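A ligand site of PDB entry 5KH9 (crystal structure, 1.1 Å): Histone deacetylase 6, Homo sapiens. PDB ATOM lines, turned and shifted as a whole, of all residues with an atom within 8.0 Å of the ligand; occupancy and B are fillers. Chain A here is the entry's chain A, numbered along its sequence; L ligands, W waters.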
ATOM      1  N   GLU A  35      32.142  21.392  -3.699  1.00  0.00           N
ATOM      2  CA  GLU A  35      31.787  22.032  -2.423  1.00  0.00           C
ATOM      3  C   GLU A  35      32.471  21.389  -1.206  1.00  0.00           C
ATOM      4  O   GLU A  35      31.823  21.218  -0.154  1.00  0.00           O
ATOM      5  CB  GLU A  35      30.237  22.166  -2.167  1.00  0.00           C
ATOM      6  CG  GLU A  35      29.873  23.277  -1.131  1.00  0.00           C
ATOM      7  CD  GLU A  35      28.447  23.286  -0.480  1.00  0.00           C
ATOM      8  OE1 GLU A  35      27.657  22.312  -0.361  1.00  0.00           O
ATOM      9  OE2 GLU A  35      28.073  24.340   0.081  1.00  0.00           O
ATOM     10  N   TRP A  37      35.081  20.953   2.105  1.00  0.00           N
ATOM     11  CA  TRP A  37      35.596  21.675   3.264  1.00  0.00           C
ATOM     12  C   TRP A  37      36.720  20.814   3.873  1.00  0.00           C
ATOM     13  O   TRP A  37      36.694  19.602   3.759  1.00  0.00           O
ATOM     14  CB  TRP A  37      34.480  21.870   4.314  1.00  0.00           C
ATOM     15  CG  TRP A  37      33.339  22.764   3.875  1.00  0.00           C
ATOM     16  CD1 TRP A  37      32.337  22.451   3.013  1.00  0.00           C
ATOM     17  CD2 TRP A  37      33.081  24.120   4.309  1.00  0.00           C
ATOM     18  NE1 TRP A  37      31.475  23.521   2.871  1.00  0.00           N
ATOM     19  CE2 TRP A  37      31.910  24.551   3.644  1.00  0.00           C
ATOM     20  CE3 TRP A  37      33.732  25.005   5.177  1.00  0.00           C
ATOM     21  CZ2 TRP A  37      31.360  25.845   3.868  1.00  0.00           C
ATOM     22  CZ3 TRP A  37      33.200  26.253   5.394  1.00  0.00           C
ATOM     23  CH2 TRP A  37      32.020  26.664   4.754  1.00  0.00           C
ATOM     24  N   GLY A  48      30.081  19.636   1.399  1.00  0.00           N
ATOM     25  CA  GLY A  48      29.176  20.594   2.006  1.00  0.00           C
ATOM     26  C   GLY A  48      27.714  20.199   2.025  1.00  0.00           C
ATOM     27  O   GLY A  48      27.266  19.193   1.422  1.00  0.00           O
ATOM     28  N   ARG A  49      26.946  21.061   2.691  1.00  0.00           N
ATOM     29  CA  ARG A  49      25.537  20.831   2.968  1.00  0.00           C
ATOM     30  C   ARG A  49      24.644  20.732   1.727  1.00  0.00           C
ATOM     31  O   ARG A  49      23.588  20.080   1.801  1.00  0.00           O
ATOM     32  CB  ARG A  49      25.024  21.962   3.904  1.00  0.00           C
ATOM     33  CG  ARG A  49      25.093  23.400   3.315  1.00  0.00           C
ATOM     34  CD  ARG A  49      25.330  24.538   4.365  1.00  0.00           C
ATOM     35  NE  ARG A  49      25.416  25.912   3.806  1.00  0.00           N
ATOM     36  CZ  ARG A  49      26.493  26.470   3.233  1.00  0.00           C
ATOM     37  NH1 ARG A  49      27.636  25.786   3.113  1.00  0.00           N
ATOM     38  NH2 ARG A  49      26.424  27.713   2.749  1.00  0.00           N
ATOM     39  N   TYR A  50      25.049  21.338   0.609  1.00  0.00           N
ATOM     40  CA  TYR A  50      24.263  21.295  -0.618  1.00  0.00           C
ATOM     41  C   TYR A  50      24.622  20.135  -1.551  1.00  0.00           C
ATOM     42  O   TYR A  50      23.922  19.923  -2.548  1.00  0.00           O
ATOM     43  CB  TYR A  50      24.327  22.649  -1.363  1.00  0.00           C
ATOM     44  CG  TYR A  50      23.771  23.810  -0.533  1.00  0.00           C
ATOM     45  CD1 TYR A  50      22.469  23.769  -0.014  1.00  0.00           C
ATOM     46  CD2 TYR A  50      24.548  24.955  -0.281  1.00  0.00           C
ATOM     47  CE1 TYR A  50      21.966  24.840   0.754  1.00  0.00           C
ATOM     48  CE2 TYR A  50      24.038  26.026   0.433  1.00  0.00           C
ATOM     49  CZ  TYR A  50      22.758  25.963   0.962  1.00  0.00           C
ATOM     50  OH  TYR A  50      22.235  27.037   1.675  1.00  0.00           O
ATOM     51  N   LEU A  56      29.007  18.017   7.723  1.00  0.00           N
ATOM     52  CA  LEU A  56      28.075  18.108   8.850  1.00  0.00           C
ATOM     53  C   LEU A  56      28.038  16.768   9.635  1.00  0.00           C
ATOM     54  O   LEU A  56      28.025  16.759  10.896  1.00  0.00           O
ATOM     55  CB  LEU A  56      26.688  18.575   8.358  1.00  0.00           C
ATOM     56  CG  LEU A  56      25.581  18.665   9.428  1.00  0.00           C
ATOM     57  CD1 LEU A  56      25.890  19.679  10.527  1.00  0.00           C
ATOM     58  CD2 LEU A  56      24.197  18.929   8.828  1.00  0.00           C
ATOM     59  N   VAL A  67      35.685  24.496  10.314  1.00  0.00           N
ATOM     60  CA  VAL A  67      35.994  23.963   8.980  1.00  0.00           C
ATOM     61  C   VAL A  67      36.257  25.122   8.000  1.00  0.00           C
ATOM     62  O   VAL A  67      35.673  26.200   8.137  1.00  0.00           O
ATOM     63  CB  VAL A  67      34.856  23.023   8.522  1.00  0.00           C
ATOM     64  CG1 VAL A  67      34.789  21.772   9.416  1.00  0.00           C
ATOM     65  CG2 VAL A  67      33.480  23.709   8.428  1.00  0.00           C
ATOM     66  N   SER A  69      36.397  26.390   3.915  1.00  0.00           N
ATOM     67  CA  SER A  69      35.839  26.099   2.574  1.00  0.00           C
ATOM     68  C   SER A  69      36.892  26.155   1.474  1.00  0.00           C
ATOM     69  O   SER A  69      37.613  27.169   1.340  1.00  0.00           O
ATOM     70  CB  SER A  69      34.753  27.102   2.245  1.00  0.00           C
ATOM     71  OG  SER A  69      34.329  26.997   0.858  1.00  0.00           O
ATOM     72  N   ASP A  72      35.609  29.287  -1.109  1.00  0.00           N
ATOM     73  CA  ASP A  72      35.808  30.725  -0.835  1.00  0.00           C
ATOM     74  C   ASP A  72      36.754  31.045   0.320  1.00  0.00           C
ATOM     75  O   ASP A  72      36.942  32.235   0.640  1.00  0.00           O
ATOM     76  CB  ASP A  72      34.458  31.474  -0.659  1.00  0.00           C
ATOM     77  CG  ASP A  72      33.717  31.089   0.618  1.00  0.00           C
ATOM     78  OD1 ASP A  72      34.233  30.274   1.385  1.00  0.00           O
ATOM     79  OD2 ASP A  72      32.590  31.592   0.868  1.00  0.00           O
ATOM     80  N   SER A  74      36.443  30.773   3.447  1.00  0.00           N
ATOM     81  CA  SER A  74      35.768  31.124   4.717  1.00  0.00           C
ATOM     82  C   SER A  74      35.896  29.998   5.742  1.00  0.00           C
ATOM     83  O   SER A  74      36.004  28.825   5.382  1.00  0.00           O
ATOM     84  CB  SER A  74      34.287  31.436   4.453  1.00  0.00           C
ATOM     85  OG  SER A  74      33.563  30.331   4.012  1.00  0.00           O
ATOM     86  N   ALA A  75      35.823  30.379   7.016  1.00  0.00           N
ATOM     87  CA  ALA A  75      35.853  29.430   8.155  1.00  0.00           C
ATOM     88  C   ALA A  75      34.526  29.491   8.923  1.00  0.00           C
ATOM     89  O   ALA A  75      34.097  30.570   9.352  1.00  0.00           O
ATOM     90  CB  ALA A  75      37.024  29.734   9.113  1.00  0.00           C
ATOM     91  N   TRP A  76      33.868  28.339   9.049  1.00  0.00           N
ATOM     92  CA  TRP A  76      32.556  28.195   9.709  1.00  0.00           C
ATOM     93  C   TRP A  76      32.718  27.389  10.992  1.00  0.00           C
ATOM     94  O   TRP A  76      33.413  26.354  11.024  1.00  0.00           O
ATOM     95  CB  TRP A  76      31.594  27.437   8.775  1.00  0.00           C
ATOM     96  CG  TRP A  76      30.190  27.148   9.321  1.00  0.00           C
ATOM     97  CD1 TRP A  76      29.689  25.949   9.751  1.00  0.00           C
ATOM     98  CD2 TRP A  76      29.094  28.093   9.406  1.00  0.00           C
ATOM     99  NE1 TRP A  76      28.376  26.071  10.117  1.00  0.00           N
ATOM    100  CE2 TRP A  76      27.973  27.371   9.901  1.00  0.00           C
ATOM    101  CE3 TRP A  76      28.936  29.455   9.077  1.00  0.00           C
ATOM    102  CZ2 TRP A  76      26.717  28.000  10.090  1.00  0.00           C
ATOM    103  CZ3 TRP A  76      27.698  30.049   9.241  1.00  0.00           C
ATOM    104  CH2 TRP A  76      26.611  29.335   9.766  1.00  0.00           C
ATOM    105  N   CYS A  77      32.055  27.859  12.082  1.00  0.00           N
ATOM    106  CA  CYS A  77      31.968  27.110  13.347  1.00  0.00           C
ATOM    107  C   CYS A  77      30.551  26.498  13.441  1.00  0.00           C
ATOM    108  O   CYS A  77      29.554  27.224  13.486  1.00  0.00           O
ATOM    109  CB  CYS A  77      32.205  27.993  14.570  1.00  0.00           C
ATOM    110  SG  CYS A  77      32.126  27.030  16.122  1.00  0.00           S
ATOM    111  N   TYR A  78      30.481  25.174  13.585  1.00  0.00           N
ATOM    112  CA  TYR A  78      29.169  24.486  13.683  1.00  0.00           C
ATOM    113  C   TYR A  78      28.473  24.695  15.052  1.00  0.00           C
ATOM    114  O   TYR A  78      27.266  24.501  15.179  1.00  0.00           O
ATOM    115  CB  TYR A  78      29.339  22.979  13.490  1.00  0.00           C
ATOM    116  CG  TYR A  78      29.575  22.555  12.030  1.00  0.00           C
ATOM    117  CD1 TYR A  78      28.549  22.569  11.081  1.00  0.00           C
ATOM    118  CD2 TYR A  78      30.851  22.153  11.593  1.00  0.00           C
ATOM    119  CE1 TYR A  78      28.763  22.189   9.752  1.00  0.00           C
ATOM    120  CE2 TYR A  78      31.065  21.749  10.269  1.00  0.00           C
ATOM    121  CZ  TYR A  78      30.037  21.773   9.343  1.00  0.00           C
ATOM    122  OH  TYR A  78      30.277  21.395   8.040  1.00  0.00           O
ATOM    123  N   GLN A  81      27.352  28.503  14.842  1.00  0.00           N
ATOM    124  CA  GLN A  81      26.598  28.697  13.603  1.00  0.00           C
ATOM    125  C   GLN A  81      26.872  30.086  13.034  1.00  0.00           C
ATOM    126  O   GLN A  81      25.968  30.888  12.780  1.00  0.00           O
ATOM    127  CB  GLN A  81      25.110  28.343  13.761  1.00  0.00           C
ATOM    128  CG  GLN A  81      24.897  26.898  14.215  1.00  0.00           C
ATOM    129  CD  GLN A  81      23.436  26.490  14.252  1.00  0.00           C
ATOM    130  OE1 GLN A  81      22.577  27.256  14.679  1.00  0.00           O
ATOM    131  NE2 GLN A  81      23.159  25.266  13.823  1.00  0.00           N
ATOM    132  N   ALA A  82      28.164  30.334  12.779  1.00  0.00           N
ATOM    133  CA  ALA A  82      28.665  31.646  12.292  1.00  0.00           C
ATOM    134  C   ALA A  82      30.021  31.473  11.641  1.00  0.00           C
ATOM    135  O   ALA A  82      30.755  30.530  11.964  1.00  0.00           O
ATOM    136  CB  ALA A  82      28.778  32.647  13.452  1.00  0.00           C
ATOM    137  N   TYR A  83      30.336  32.417  10.749  1.00  0.00           N
ATOM    138  CA  TYR A  83      31.688  32.539  10.227  1.00  0.00           C
ATOM    139  C   TYR A  83      32.593  33.239  11.252  1.00  0.00           C
ATOM    140  O   TYR A  83      32.127  34.106  12.023  1.00  0.00           O
ATOM    141  CB  TYR A  83      31.693  33.323   8.922  1.00  0.00           C
ATOM    142  CG  TYR A  83      30.992  32.634   7.785  1.00  0.00           C
ATOM    143  CD1 TYR A  83      31.600  31.588   7.096  1.00  0.00           C
ATOM    144  CD2 TYR A  83      29.700  33.019   7.409  1.00  0.00           C
ATOM    145  CE1 TYR A  83      30.958  30.981   5.990  1.00  0.00           C
ATOM    146  CE2 TYR A  83      29.039  32.395   6.358  1.00  0.00           C
ATOM    147  CZ  TYR A  83      29.651  31.388   5.658  1.00  0.00           C
ATOM    148  OH  TYR A  83      28.981  30.833   4.579  1.00  0.00           O
HETATM  149  O1  LIG L   1      23.674  26.768   7.702  1.00  0.00           O
HETATM  150  C1  LIG L   1      24.795  27.104   7.255  1.00  0.00           C
HETATM  151  N1  LIG L   1      25.793  26.182   7.271  1.00  0.00           N
HETATM  152  N2  LIG L   1      27.063  26.414   6.789  1.00  0.00           N
HETATM  153  C2  LIG L   1      27.326  27.592   6.347  1.00  0.00           C
HETATM  154  C3  LIG L   1      28.714  27.843   5.841  1.00  0.00           C
HETATM  155  N3  LIG L   1      25.069  28.354   6.759  1.00  0.00           N
HETATM  156  C4  LIG L   1      26.302  28.617   6.329  1.00  0.00           C
HETATM  157  N4  LIG L   1      26.426  29.797   5.681  1.00  0.00           N
HETATM  158  C5  LIG L   1      25.602  30.950   5.670  1.00  0.00           C
HETATM  159  C6  LIG L   1      25.784  31.859   4.628  1.00  0.00           C
HETATM  160  C7  LIG L   1      25.001  32.996   4.560  1.00  0.00           C
HETATM  161  C8  LIG L   1      24.046  33.289   5.539  1.00  0.00           C
HETATM  162  C9  LIG L   1      23.207  34.551   5.414  1.00  0.00           C
HETATM  163  C10 LIG L   1      21.848  34.277   4.739  1.00  0.00           C
HETATM  164  C11 LIG L   1      23.045  35.311   6.735  1.00  0.00           C
HETATM  165  C12 LIG L   1      23.917  32.400   6.607  1.00  0.00           C
HETATM  166  C13 LIG L   1      24.689  31.255   6.682  1.00  0.00           C
HETATM  167  O   HOH W   1      22.699  26.692   4.421  1.00  0.00           O
HETATM  168  O   HOH W   2      25.767  23.361   7.889  1.00  0.00           O
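OH of Tyr 83 lies within hydrogen-bond range of N4 of the ligand (3.0 Å). A nitrogen (N2) of the ligand sits at hydrogen-bond distance from the guanidinium group (NE) of Arg 49 (3.4 Å).
The side-chain carboxylate (OE2) of Glu 35 is in salt-bridge range of the guanidinium group (NH1) of Arg 49 (3.4 Å). N of Trp 76 lies within hydrogen-bond range of O of Val 67, at 2.9 Å.
Merely in contact with the ligand: Trp 37 (3.7 Å) and Trp 76 (3.4 Å).
Water W1 lies within hydrogen-bond range of the side-chain hydroxyl of Tyr 50, the guanidinium group of Arg 49 and an oxygen (O1) of the ligand.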
